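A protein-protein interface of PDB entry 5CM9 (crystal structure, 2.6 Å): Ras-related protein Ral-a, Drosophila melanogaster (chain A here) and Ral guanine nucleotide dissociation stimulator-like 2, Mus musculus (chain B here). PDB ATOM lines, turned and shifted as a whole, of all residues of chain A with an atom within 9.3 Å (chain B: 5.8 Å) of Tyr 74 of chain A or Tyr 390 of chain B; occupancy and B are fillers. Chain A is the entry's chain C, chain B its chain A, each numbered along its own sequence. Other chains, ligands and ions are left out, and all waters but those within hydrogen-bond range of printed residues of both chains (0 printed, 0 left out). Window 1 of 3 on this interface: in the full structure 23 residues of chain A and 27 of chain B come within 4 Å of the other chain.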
ATOM      1  N   ASP A  67      -2.902  -7.387  23.614  1.00  0.00           N
ATOM      2  CA  ASP A  67      -3.836  -7.335  22.490  1.00  0.00           C
ATOM      3  C   ASP A  67      -4.578  -8.643  22.246  1.00  0.00           C
ATOM      4  O   ASP A  67      -4.021  -9.730  22.407  1.00  0.00           O
ATOM      5  CB  ASP A  67      -3.108  -6.915  21.207  1.00  0.00           C
ATOM      6  CG  ASP A  67      -3.416  -5.479  20.797  1.00  0.00           C
ATOM      7  OD1 ASP A  67      -3.800  -4.662  21.665  1.00  0.00           O
ATOM      8  OD2 ASP A  67      -3.276  -5.167  19.594  1.00  0.00           O
ATOM      9  N   THR A  68      -5.842  -8.518  21.856  1.00  0.00           N
ATOM     10  CA  THR A  68      -6.620  -9.648  21.362  1.00  0.00           C
ATOM     11  C   THR A  68      -6.547  -9.665  19.833  1.00  0.00           C
ATOM     12  O   THR A  68      -7.400 -10.254  19.166  1.00  0.00           O
ATOM     13  CB  THR A  68      -8.100  -9.567  21.810  1.00  0.00           C
ATOM     14  OG1 THR A  68      -8.659  -8.311  21.401  1.00  0.00           O
ATOM     15  CG2 THR A  68      -8.223  -9.714  23.325  1.00  0.00           C
ATOM     16  N   ALA A  69      -5.515  -9.012  19.295  1.00  0.00           N
ATOM     17  CA  ALA A  69      -5.337  -8.840  17.855  1.00  0.00           C
ATOM     18  C   ALA A  69      -5.248 -10.177  17.129  1.00  0.00           C
ATOM     19  O   ALA A  69      -4.492 -11.059  17.532  1.00  0.00           O
ATOM     20  CB  ALA A  69      -4.104  -7.992  17.573  1.00  0.00           C
ATOM     21  N   GLY A  70      -6.043 -10.319  16.074  1.00  0.00           N
ATOM     22  CA  GLY A  70      -6.098 -11.552  15.293  1.00  0.00           C
ATOM     23  C   GLY A  70      -6.818 -12.700  15.977  1.00  0.00           C
ATOM     24  O   GLY A  70      -7.246 -13.647  15.318  1.00  0.00           O
ATOM     25  N   GLN A  71      -6.958 -12.611  17.296  1.00  0.00           N
ATOM     26  CA  GLN A  71      -7.497 -13.700  18.108  1.00  0.00           C
ATOM     27  C   GLN A  71      -8.915 -13.425  18.620  1.00  0.00           C
ATOM     28  O   GLN A  71      -9.351 -14.018  19.608  1.00  0.00           O
ATOM     29  CB  GLN A  71      -6.564 -13.982  19.291  1.00  0.00           C
ATOM     30  CG  GLN A  71      -5.166 -14.436  18.904  1.00  0.00           C
ATOM     31  CD  GLN A  71      -4.264 -14.636  20.111  1.00  0.00           C
ATOM     32  OE1 GLN A  71      -3.399 -13.812  20.394  1.00  0.00           O
ATOM     33  NE2 GLN A  71      -4.475 -15.729  20.837  1.00  0.00           N
ATOM     34  N   GLU A  72      -9.635 -12.541  17.932  1.00  0.00           N
ATOM     35  CA  GLU A  72     -10.953 -12.077  18.378  1.00  0.00           C
ATOM     36  C   GLU A  72     -12.058 -13.129  18.255  1.00  0.00           C
ATOM     37  O   GLU A  72     -13.026 -13.106  19.017  1.00  0.00           O
ATOM     38  CB  GLU A  72     -11.374 -10.808  17.621  1.00  0.00           C
ATOM     39  CG  GLU A  72     -10.424  -9.618  17.749  1.00  0.00           C
ATOM     40  CD  GLU A  72      -9.316  -9.620  16.702  1.00  0.00           C
ATOM     41  OE1 GLU A  72      -9.290 -10.527  15.839  1.00  0.00           O
ATOM     42  OE2 GLU A  72      -8.466  -8.705  16.741  1.00  0.00           O
ATOM     43  N   ASP A  73     -11.918 -14.041  17.296  1.00  0.00           N
ATOM     44  CA  ASP A  73     -12.940 -15.066  17.054  1.00  0.00           C
ATOM     45  C   ASP A  73     -12.746 -16.322  17.912  1.00  0.00           C
ATOM     46  O   ASP A  73     -13.563 -17.242  17.866  1.00  0.00           O
ATOM     47  CB  ASP A  73     -13.005 -15.437  15.567  1.00  0.00           C
ATOM     48  CG  ASP A  73     -13.306 -14.246  14.672  1.00  0.00           C
ATOM     49  OD1 ASP A  73     -13.526 -13.131  15.190  1.00  0.00           O
ATOM     50  OD2 ASP A  73     -13.315 -14.425  13.440  1.00  0.00           O
ATOM     51  N   TYR A  74     -11.669 -16.355  18.689  1.00  0.00           N
ATOM     52  CA  TYR A  74     -11.432 -17.457  19.607  1.00  0.00           C
ATOM     53  C   TYR A  74     -12.217 -17.232  20.892  1.00  0.00           C
ATOM     54  O   TYR A  74     -11.998 -16.248  21.601  1.00  0.00           O
ATOM     55  CB  TYR A  74      -9.940 -17.612  19.906  1.00  0.00           C
ATOM     56  CG  TYR A  74      -9.116 -18.127  18.750  1.00  0.00           C
ATOM     57  CD1 TYR A  74      -8.150 -17.321  18.141  1.00  0.00           C
ATOM     58  CD2 TYR A  74      -9.291 -19.422  18.266  1.00  0.00           C
ATOM     59  CE1 TYR A  74      -7.381 -17.794  17.079  1.00  0.00           C
ATOM     60  CE2 TYR A  74      -8.532 -19.901  17.205  1.00  0.00           C
ATOM     61  CZ  TYR A  74      -7.582 -19.082  16.617  1.00  0.00           C
ATOM     62  OH  TYR A  74      -6.837 -19.561  15.569  1.00  0.00           O
ATOM     63  N   ALA A  75     -13.129 -18.154  21.182  1.00  0.00           N
ATOM     64  CA  ALA A  75     -14.045 -18.026  22.313  1.00  0.00           C
ATOM     65  C   ALA A  75     -13.339 -17.994  23.674  1.00  0.00           C
ATOM     66  O   ALA A  75     -13.284 -16.949  24.324  1.00  0.00           O
ATOM     67  CB  ALA A  75     -15.101 -19.138  22.272  1.00  0.00           C
ATOM     68  N   ALA A  76     -12.784 -19.134  24.081  1.00  0.00           N
ATOM     69  CA  ALA A  76     -12.216 -19.307  25.420  1.00  0.00           C
ATOM     70  C   ALA A  76     -10.942 -18.497  25.694  1.00  0.00           C
ATOM     71  O   ALA A  76     -10.584 -18.277  26.852  1.00  0.00           O
ATOM     72  CB  ALA A  76     -11.976 -20.787  25.691  1.00  0.00           C
ATOM     73  N   ILE A  77     -10.270 -18.052  24.632  1.00  0.00           N
ATOM     74  CA  ILE A  77      -8.999 -17.331  24.742  1.00  0.00           C
ATOM     75  C   ILE A  77      -9.138 -15.997  25.477  1.00  0.00           C
ATOM     76  O   ILE A  77      -8.472 -15.781  26.491  1.00  0.00           O
ATOM     77  CB  ILE A  77      -8.327 -17.126  23.353  1.00  0.00           C
ATOM     78  CG1 ILE A  77      -8.149 -18.463  22.624  1.00  0.00           C
ATOM     79  CG2 ILE A  77      -6.980 -16.415  23.477  1.00  0.00           C
ATOM     80  CD1 ILE A  77      -7.572 -19.578  23.463  1.00  0.00           C
ATOM     81  N   ARG A  78     -10.009 -15.119  24.975  1.00  0.00           N
ATOM     82  CA  ARG A  78     -10.222 -13.796  25.578  1.00  0.00           C
ATOM     83  C   ARG A  78     -10.648 -13.879  27.048  1.00  0.00           C
ATOM     84  O   ARG A  78     -10.297 -13.017  27.851  1.00  0.00           O
ATOM     85  CB  ARG A  78     -11.209 -12.953  24.756  1.00  0.00           C
ATOM     86  CG  ARG A  78     -12.613 -13.526  24.625  1.00  0.00           C
ATOM     87  CD  ARG A  78     -13.423 -12.798  23.561  1.00  0.00           C
ATOM     88  NE  ARG A  78     -14.526 -13.629  23.080  1.00  0.00           N
ATOM     89  CZ  ARG A  78     -15.152 -13.463  21.917  1.00  0.00           C
ATOM     90  NH1 ARG A  78     -14.797 -12.482  21.094  1.00  0.00           N
ATOM     91  NH2 ARG A  78     -16.137 -14.286  21.574  1.00  0.00           N
ATOM     92  N   ASP A  79     -11.386 -14.936  27.384  1.00  0.00           N
ATOM     93  CA  ASP A  79     -11.798 -15.226  28.757  1.00  0.00           C
ATOM     94  C   ASP A  79     -10.593 -15.283  29.696  1.00  0.00           C
ATOM     95  O   ASP A  79     -10.650 -14.791  30.825  1.00  0.00           O
ATOM     96  CB  ASP A  79     -12.560 -16.555  28.797  1.00  0.00           C
ATOM     97  CG  ASP A  79     -13.387 -16.731  30.056  1.00  0.00           C
ATOM     98  OD1 ASP A  79     -12.839 -16.596  31.171  1.00  0.00           O
ATOM     99  OD2 ASP A  79     -14.594 -17.025  29.929  1.00  0.00           O
ATOM    100  N   ASN A  80      -9.505 -15.879  29.212  1.00  0.00           N
ATOM    101  CA  ASN A  80      -8.276 -16.025  29.987  1.00  0.00           C
ATOM    102  C   ASN A  80      -7.572 -14.685  30.163  1.00  0.00           C
ATOM    103  O   ASN A  80      -7.039 -14.397  31.236  1.00  0.00           O
ATOM    104  CB  ASN A  80      -7.334 -17.034  29.324  1.00  0.00           C
ATOM    105  CG  ASN A  80      -7.887 -18.460  29.319  1.00  0.00           C
ATOM    106  OD1 ASN A  80      -7.126 -19.417  29.190  1.00  0.00           O
ATOM    107  ND2 ASN A  80      -9.203 -18.605  29.452  1.00  0.00           N
ATOM    108  N   TYR A  81      -7.579 -13.876  29.102  1.00  0.00           N
ATOM    109  CA  TYR A  81      -7.058 -12.509  29.150  1.00  0.00           C
ATOM    110  C   TYR A  81      -7.791 -11.682  30.207  1.00  0.00           C
ATOM    111  O   TYR A  81      -7.154 -11.031  31.039  1.00  0.00           O
ATOM    112  CB  TYR A  81      -7.168 -11.821  27.781  1.00  0.00           C
ATOM    113  CG  TYR A  81      -6.151 -12.273  26.748  1.00  0.00           C
ATOM    114  CD1 TYR A  81      -6.471 -13.253  25.808  1.00  0.00           C
ATOM    115  CD2 TYR A  81      -4.874 -11.709  26.700  1.00  0.00           C
ATOM    116  CE1 TYR A  81      -5.542 -13.670  24.851  1.00  0.00           C
ATOM    117  CE2 TYR A  81      -3.936 -12.124  25.745  1.00  0.00           C
ATOM    118  CZ  TYR A  81      -4.279 -13.104  24.824  1.00  0.00           C
ATOM    119  OH  TYR A  81      -3.361 -13.515  23.878  1.00  0.00           O
ATOM    120  N   PHE A  82      -9.123 -11.738  30.190  1.00  0.00           N
ATOM    121  CA  PHE A  82      -9.949 -10.900  31.066  1.00  0.00           C
ATOM    122  C   PHE A  82      -9.836 -11.254  32.555  1.00  0.00           C
ATOM    123  O   PHE A  82     -10.164 -10.435  33.412  1.00  0.00           O
ATOM    124  CB  PHE A  82     -11.423 -10.899  30.627  1.00  0.00           C
ATOM    125  CG  PHE A  82     -11.647 -10.508  29.185  1.00  0.00           C
ATOM    126  CD1 PHE A  82     -10.692  -9.787  28.472  1.00  0.00           C
ATOM    127  CD2 PHE A  82     -12.836 -10.842  28.550  1.00  0.00           C
ATOM    128  CE1 PHE A  82     -10.907  -9.434  27.144  1.00  0.00           C
ATOM    129  CE2 PHE A  82     -13.065 -10.484  27.223  1.00  0.00           C
ATOM    130  CZ  PHE A  82     -12.098  -9.777  26.522  1.00  0.00           C
ATOM    131  N   PHE A 106     -18.683  -7.449  24.051  1.00  0.00           N
ATOM    132  CA  PHE A 106     -17.396  -7.352  24.745  1.00  0.00           C
ATOM    133  C   PHE A 106     -17.564  -6.834  26.172  1.00  0.00           C
ATOM    134  O   PHE A 106     -16.874  -7.283  27.084  1.00  0.00           O
ATOM    135  CB  PHE A 106     -16.410  -6.470  23.970  1.00  0.00           C
ATOM    136  CG  PHE A 106     -16.146  -6.933  22.561  1.00  0.00           C
ATOM    137  CD1 PHE A 106     -16.318  -6.063  21.489  1.00  0.00           C
ATOM    138  CD2 PHE A 106     -15.724  -8.236  22.301  1.00  0.00           C
ATOM    139  CE1 PHE A 106     -16.081  -6.481  20.182  1.00  0.00           C
ATOM    140  CE2 PHE A 106     -15.484  -8.666  20.997  1.00  0.00           C
ATOM    141  CZ  PHE A 106     -15.662  -7.785  19.934  1.00  0.00           C
ATOM    142  N   GLN A 109     -19.010  -9.918  28.069  1.00  0.00           N
ATOM    143  CA  GLN A 109     -17.969 -10.924  28.309  1.00  0.00           C
ATOM    144  C   GLN A 109     -17.098 -10.561  29.508  1.00  0.00           C
ATOM    145  O   GLN A 109     -16.780 -11.420  30.334  1.00  0.00           O
ATOM    146  CB  GLN A 109     -17.093 -11.105  27.062  1.00  0.00           C
ATOM    147  CG  GLN A 109     -17.793 -11.770  25.872  1.00  0.00           C
ATOM    148  CD  GLN A 109     -17.190 -11.378  24.525  1.00  0.00           C
ATOM    149  OE1 GLN A 109     -16.128 -10.753  24.458  1.00  0.00           O
ATOM    150  NE2 GLN A 109     -17.878 -11.740  23.444  1.00  0.00           N
ATOM    151  N   VAL B 246      -8.811 -20.339   7.259  1.00  0.00           N
ATOM    152  CA  VAL B 246      -8.466 -19.839   8.588  1.00  0.00           C
ATOM    153  C   VAL B 246      -9.672 -19.943   9.521  1.00  0.00           C
ATOM    154  O   VAL B 246      -9.546 -20.435  10.642  1.00  0.00           O
ATOM    155  CB  VAL B 246      -7.960 -18.380   8.551  1.00  0.00           C
ATOM    156  CG1 VAL B 246      -7.477 -17.950   9.928  1.00  0.00           C
ATOM    157  CG2 VAL B 246      -6.847 -18.220   7.520  1.00  0.00           C
ATOM    158  N   THR B 249     -10.376 -23.434  10.770  1.00  0.00           N
ATOM    159  CA  THR B 249      -9.485 -23.721  11.896  1.00  0.00           C
ATOM    160  C   THR B 249     -10.054 -23.201  13.221  1.00  0.00           C
ATOM    161  O   THR B 249     -10.031 -23.905  14.236  1.00  0.00           O
ATOM    162  CB  THR B 249      -8.059 -23.136  11.622  1.00  0.00           C
ATOM    163  OG1 THR B 249      -7.284 -24.092  10.890  1.00  0.00           O
ATOM    164  CG2 THR B 249      -7.319 -22.768  12.906  1.00  0.00           C
ATOM    165  N   VAL B 250     -10.563 -21.969  13.190  1.00  0.00           N
ATOM    166  CA  VAL B 250     -11.122 -21.292  14.361  1.00  0.00           C
ATOM    167  C   VAL B 250     -12.414 -21.980  14.823  1.00  0.00           C
ATOM    168  O   VAL B 250     -12.607 -22.225  16.018  1.00  0.00           O
ATOM    169  CB  VAL B 250     -11.373 -19.783  14.066  1.00  0.00           C
ATOM    170  CG1 VAL B 250     -12.044 -19.091  15.246  1.00  0.00           C
ATOM    171  CG2 VAL B 250     -10.060 -19.076  13.716  1.00  0.00           C
ATOM    172  N   PHE B 253     -11.470 -25.041  16.721  1.00  0.00           N
ATOM    173  CA  PHE B 253     -11.002 -24.636  18.035  1.00  0.00           C
ATOM    174  C   PHE B 253     -12.208 -24.336  18.941  1.00  0.00           C
ATOM    175  O   PHE B 253     -12.232 -24.746  20.100  1.00  0.00           O
ATOM    176  CB  PHE B 253     -10.079 -23.422  17.915  1.00  0.00           C
ATOM    177  CG  PHE B 253      -9.413 -23.030  19.202  1.00  0.00           C
ATOM    178  CD1 PHE B 253      -8.085 -23.354  19.432  1.00  0.00           C
ATOM    179  CD2 PHE B 253     -10.109 -22.323  20.178  1.00  0.00           C
ATOM    180  CE1 PHE B 253      -7.463 -22.989  20.616  1.00  0.00           C
ATOM    181  CE2 PHE B 253      -9.495 -21.958  21.365  1.00  0.00           C
ATOM    182  CZ  PHE B 253      -8.170 -22.291  21.580  1.00  0.00           C
ATOM    183  N   ASN B 254     -13.210 -23.647  18.401  1.00  0.00           N
ATOM    184  CA  ASN B 254     -14.409 -23.298  19.169  1.00  0.00           C
ATOM    185  C   ASN B 254     -15.360 -24.466  19.449  1.00  0.00           C
ATOM    186  O   ASN B 254     -16.023 -24.496  20.489  1.00  0.00           O
ATOM    187  CB  ASN B 254     -15.155 -22.126  18.522  1.00  0.00           C
ATOM    188  CG  ASN B 254     -14.414 -20.800  18.675  1.00  0.00           C
ATOM    189  OD1 ASN B 254     -13.513 -20.655  19.510  1.00  0.00           O
ATOM    190  ND2 ASN B 254     -14.793 -19.827  17.862  1.00  0.00           N
ATOM    191  N   PHE B 307      -1.068 -28.536  19.581  1.00  0.00           N
ATOM    192  CA  PHE B 307      -1.159 -27.435  20.534  1.00  0.00           C
ATOM    193  C   PHE B 307      -2.454 -26.645  20.390  1.00  0.00           C
ATOM    194  O   PHE B 307      -2.906 -26.009  21.342  1.00  0.00           O
ATOM    195  CB  PHE B 307       0.055 -26.512  20.415  1.00  0.00           C
ATOM    196  CG  PHE B 307       1.373 -27.209  20.630  1.00  0.00           C
ATOM    197  CD1 PHE B 307       2.105 -27.694  19.548  1.00  0.00           C
ATOM    198  CD2 PHE B 307       1.887 -27.375  21.909  1.00  0.00           C
ATOM    199  CE1 PHE B 307       3.326 -28.339  19.739  1.00  0.00           C
ATOM    200  CE2 PHE B 307       3.111 -28.021  22.112  1.00  0.00           C
ATOM    201  CZ  PHE B 307       3.831 -28.501  21.025  1.00  0.00           C
ATOM    202  N   SER B 308      -3.053 -26.694  19.206  1.00  0.00           N
ATOM    203  CA  SER B 308      -4.340 -26.052  18.973  1.00  0.00           C
ATOM    204  C   SER B 308      -5.407 -26.582  19.938  1.00  0.00           C
ATOM    205  O   SER B 308      -6.112 -25.798  20.574  1.00  0.00           O
ATOM    206  CB  SER B 308      -4.781 -26.238  17.521  1.00  0.00           C
ATOM    207  OG  SER B 308      -5.975 -25.525  17.260  1.00  0.00           O
ATOM    208  N   TYR B 311      -4.673 -25.967  23.731  1.00  0.00           N
ATOM    209  CA  TYR B 311      -5.080 -24.613  24.089  1.00  0.00           C
ATOM    210  C   TYR B 311      -6.599 -24.438  24.115  1.00  0.00           C
ATOM    211  O   TYR B 311      -7.116 -23.655  24.905  1.00  0.00           O
ATOM    212  CB  TYR B 311      -4.406 -23.582  23.170  1.00  0.00           C
ATOM    213  CG  TYR B 311      -4.400 -22.161  23.704  1.00  0.00           C
ATOM    214  CD1 TYR B 311      -4.414 -21.900  25.083  1.00  0.00           C
ATOM    215  CD2 TYR B 311      -4.356 -21.074  22.829  1.00  0.00           C
ATOM    216  CE1 TYR B 311      -4.406 -20.588  25.577  1.00  0.00           C
ATOM    217  CE2 TYR B 311      -4.345 -19.753  23.309  1.00  0.00           C
ATOM    218  CZ  TYR B 311      -4.373 -19.519  24.682  1.00  0.00           C
ATOM    219  OH  TYR B 311      -4.362 -18.220  25.155  1.00  0.00           O
ATOM    220  N   PHE B 347       0.872 -22.141  28.421  1.00  0.00           N
ATOM    221  CA  PHE B 347       0.101 -21.005  27.920  1.00  0.00           C
ATOM    222  C   PHE B 347      -0.146 -19.973  29.016  1.00  0.00           C
ATOM    223  O   PHE B 347       0.075 -18.778  28.818  1.00  0.00           O
ATOM    224  CB  PHE B 347      -1.232 -21.481  27.339  1.00  0.00           C
ATOM    225  CG  PHE B 347      -1.089 -22.337  26.110  1.00  0.00           C
ATOM    226  CD1 PHE B 347      -0.975 -21.752  24.846  1.00  0.00           C
ATOM    227  CD2 PHE B 347      -1.079 -23.726  26.211  1.00  0.00           C
ATOM    228  CE1 PHE B 347      -0.848 -22.542  23.698  1.00  0.00           C
ATOM    229  CE2 PHE B 347      -0.951 -24.524  25.069  1.00  0.00           C
ATOM    230  CZ  PHE B 347      -0.835 -23.929  23.811  1.00  0.00           C
ATOM    231  N   VAL B 388       0.336 -29.672  15.158  1.00  0.00           N
ATOM    232  CA  VAL B 388      -0.681 -28.705  14.802  1.00  0.00           C
ATOM    233  C   VAL B 388      -0.490 -27.545  15.760  1.00  0.00           C
ATOM    234  O   VAL B 388      -0.751 -27.680  16.958  1.00  0.00           O
ATOM    235  CB  VAL B 388      -2.124 -29.252  14.909  1.00  0.00           C
ATOM    236  CG1 VAL B 388      -3.119 -28.234  14.351  1.00  0.00           C
ATOM    237  CG2 VAL B 388      -2.267 -30.578  14.186  1.00  0.00           C
ATOM    238  N   PRO B 389       0.005 -26.410  15.242  1.00  0.00           N
ATOM    239  CA  PRO B 389       0.228 -25.254  16.091  1.00  0.00           C
ATOM    240  C   PRO B 389      -1.083 -24.568  16.418  1.00  0.00           C
ATOM    241  O   PRO B 389      -2.075 -24.747  15.707  1.00  0.00           O
ATOM    242  CB  PRO B 389       1.083 -24.344  15.211  1.00  0.00           C
ATOM    243  CG  PRO B 389       0.675 -24.679  13.837  1.00  0.00           C
ATOM    244  CD  PRO B 389       0.395 -26.148  13.846  1.00  0.00           C
ATOM    245  N   TYR B 390      -1.085 -23.809  17.506  1.00  0.00           N
ATOM    246  CA  TYR B 390      -2.168 -22.888  17.758  1.00  0.00           C
ATOM    247  C   TYR B 390      -1.982 -21.712  16.816  1.00  0.00           C
ATOM    248  O   TYR B 390      -1.101 -20.877  17.018  1.00  0.00           O
ATOM    249  CB  TYR B 390      -2.192 -22.423  19.219  1.00  0.00           C
ATOM    250  CG  TYR B 390      -3.124 -21.253  19.449  1.00  0.00           C
ATOM    251  CD1 TYR B 390      -4.490 -21.358  19.178  1.00  0.00           C
ATOM    252  CD2 TYR B 390      -2.639 -20.034  19.922  1.00  0.00           C
ATOM    253  CE1 TYR B 390      -5.349 -20.280  19.376  1.00  0.00           C
ATOM    254  CE2 TYR B 390      -3.488 -18.953  20.127  1.00  0.00           C
ATOM    255  CZ  TYR B 390      -4.841 -19.081  19.853  1.00  0.00           C
ATOM    256  OH  TYR B 390      -5.685 -18.014  20.053  1.00  0.00           O
ATOM    257  N   LEU B 391      -2.783 -21.682  15.758  1.00  0.00           N
ATOM    258  CA  LEU B 391      -2.861 -20.516  14.900  1.00  0.00           C
ATOM    259  C   LEU B 391      -3.566 -19.481  15.752  1.00  0.00           C
ATOM    260  O   LEU B 391      -4.502 -19.807  16.468  1.00  0.00           O
ATOM    261  CB  LEU B 391      -3.679 -20.827  13.647  1.00  0.00           C
ATOM    262  CG  LEU B 391      -3.623 -19.841  12.474  1.00  0.00           C
ATOM    263  CD1 LEU B 391      -2.271 -19.870  11.768  1.00  0.00           C
ATOM    264  CD2 LEU B 391      -4.732 -20.136  11.478  1.00  0.00           C
ATOM    265  N   GLY B 392      -3.107 -18.243  15.714  1.00  0.00           N
ATOM    266  CA  GLY B 392      -3.662 -17.238  16.614  1.00  0.00           C
ATOM    267  C   GLY B 392      -2.505 -16.411  17.097  1.00  0.00           C
ATOM    268  O   GLY B 392      -2.553 -15.183  17.067  1.00  0.00           O
ATOM    269  N   THR B 393      -1.458 -17.112  17.529  1.00  0.00           N
ATOM    270  CA  THR B 393      -0.155 -16.512  17.764  1.00  0.00           C
ATOM    271  C   THR B 393       0.354 -15.993  16.424  1.00  0.00           C
ATOM    272  O   THR B 393       0.874 -14.884  16.339  1.00  0.00           O
ATOM    273  CB  THR B 393       0.841 -17.535  18.352  1.00  0.00           C
ATOM    274  OG1 THR B 393       0.203 -18.286  19.393  1.00  0.00           O
ATOM    275  CG2 THR B 393       2.064 -16.835  18.921  1.00  0.00           C
ATOM    276  N   PHE B 394       0.175 -16.797  15.378  1.00  0.00           N
ATOM    277  CA  PHE B 394       0.541 -16.405  14.023  1.00  0.00           C
ATOM    278  C   PHE B 394      -0.330 -15.265  13.518  1.00  0.00           C
ATOM    279  O   PHE B 394       0.182 -14.264  13.013  1.00  0.00           O
ATOM    280  CB  PHE B 394       0.483 -17.608  13.079  1.00  0.00           C
ATOM    281  CG  PHE B 394       1.557 -18.620  13.339  1.00  0.00           C
ATOM    282  CD1 PHE B 394       1.375 -19.618  14.292  1.00  0.00           C
ATOM    283  CD2 PHE B 394       2.766 -18.559  12.651  1.00  0.00           C
ATOM    284  CE1 PHE B 394       2.374 -20.546  14.553  1.00  0.00           C
ATOM    285  CE2 PHE B 394       3.775 -19.483  12.900  1.00  0.00           C
ATOM    286  CZ  PHE B 394       3.579 -20.480  13.854  1.00  0.00           C
ATOM    287  N   LEU B 395      -1.643 -15.410  13.678  1.00  0.00           N
ATOM    288  CA  LEU B 395      -2.594 -14.378  13.271  1.00  0.00           C
ATOM    289  C   LEU B 395      -2.316 -13.047  13.980  1.00  0.00           C
ATOM    290  O   LEU B 395      -2.320 -11.995  13.344  1.00  0.00           O
ATOM    291  CB  LEU B 395      -4.030 -14.847  13.507  1.00  0.00           C
ATOM    292  CG  LEU B 395      -4.508 -16.007  12.625  1.00  0.00           C
ATOM    293  CD1 LEU B 395      -5.701 -16.733  13.252  1.00  0.00           C
ATOM    294  CD2 LEU B 395      -4.834 -15.548  11.207  1.00  0.00           C
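The backbone carbonyl oxygen of Asp 73 of chain A is in hydrogen-bond range of the side-chain amide nitrogen of Asn 254 of chain B (2.9 Å).
OD1 of Asn 254 of chain B sits at hydrogen-bond distance from N of Ala 75 of chain A (3.0 Å).
The side-chain hydroxyl of Tyr 390 of chain B sits at hydrogen-bond distance from the side-chain amide nitrogen of Gln 71 of chain A (2.7 Å).
The backbone carbonyl oxygen (O) of Leu 391 of chain B is in hydrogen-bond range of the side-chain hydroxyl (OH) of Tyr 74 of chain A, at 2.5 Å.
The side-chain carboxylate (OE2) of Glu 72 of chain A is in hydrogen-bond range of the backbone NH (N) of Gly 70 of chain A, at 3.0 Å.
OE1 of Gln 71 of chain A sits at hydrogen-bond distance from OH of Tyr 81 of chain A.
Gly 70 of chain A touches Leu 395 of chain B.
Gln 71 of chain A touches Gly 392 of chain B.
Tyr 74 of chain A touches Val 250 of chain B (OH to CG2, 3.7 Å).
OD1 of Asn 254 of chain B touches CA of Tyr 74 of chain A, at 3.8 Å.
Tyr 74 of chain A touches Tyr 390 of chain B.
Gly 392 of chain B touches Tyr 74 of chain A.
Leu 395 of chain B touches Tyr 74 of chain A (CD1 to OH, 3.8 Å).
Ile 77 of chain A touches Phe 253 of chain B (CD1 to CZ, 3.4 Å).
Ile 77 of chain A touches Tyr 311 of chain B (CD1 to CE2, 3.2 Å).
OH of Tyr 390 of chain B touches CG1 of Ile 77 of chain A, at 3.6 Å.
Printed residues of chain B within 4 Å of Gly 70 of chain A: Leu 395 (3.9 Å).
Of the printed residues of chain B, Gln 71 of chain A touches Tyr 390 and Gly 392.
Tyr 74 of chain A touches just these residues of chain B: Val 250, Phe 253, Asn 254, Tyr 390, Leu 391, Gly 392 and Leu 395.
Tyr 81 of chain A touches none of the printed residues of chain B.
Val 250 of chain B touches two residues of chain A.
Of the printed residues of chain A, Asn 254 of chain B touches Asp 73 (2.9 Å), Tyr 74 (3.8 Å) and Ala 75 (3.0 Å).
Of the printed residues of chain A, Leu 391 of chain B touches Tyr 74 (2.5 Å).
Gly 392 of chain B touches two residues of chain A.
Phe 394 of chain B touches none of the printed residues of chain A.
Of the printed residues of chain A, Leu 395 of chain B touches Gly 70 and Tyr 74.
The nearest residue of chain A that does not touch Tyr 390 of chain B is Tyr 81 of chain A (6.3 Å).
The nearest printed residue of chain A that does not touch Asn 254 of chain B is Ala 76 of chain A (4.9 Å).
Among the printed residues, 16 pairs touch across the chains.
Among the printed residues, no Asp or Glu carboxylate lies within 4 Å of a Lys or Arg side-chain nitrogen of the other chain.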
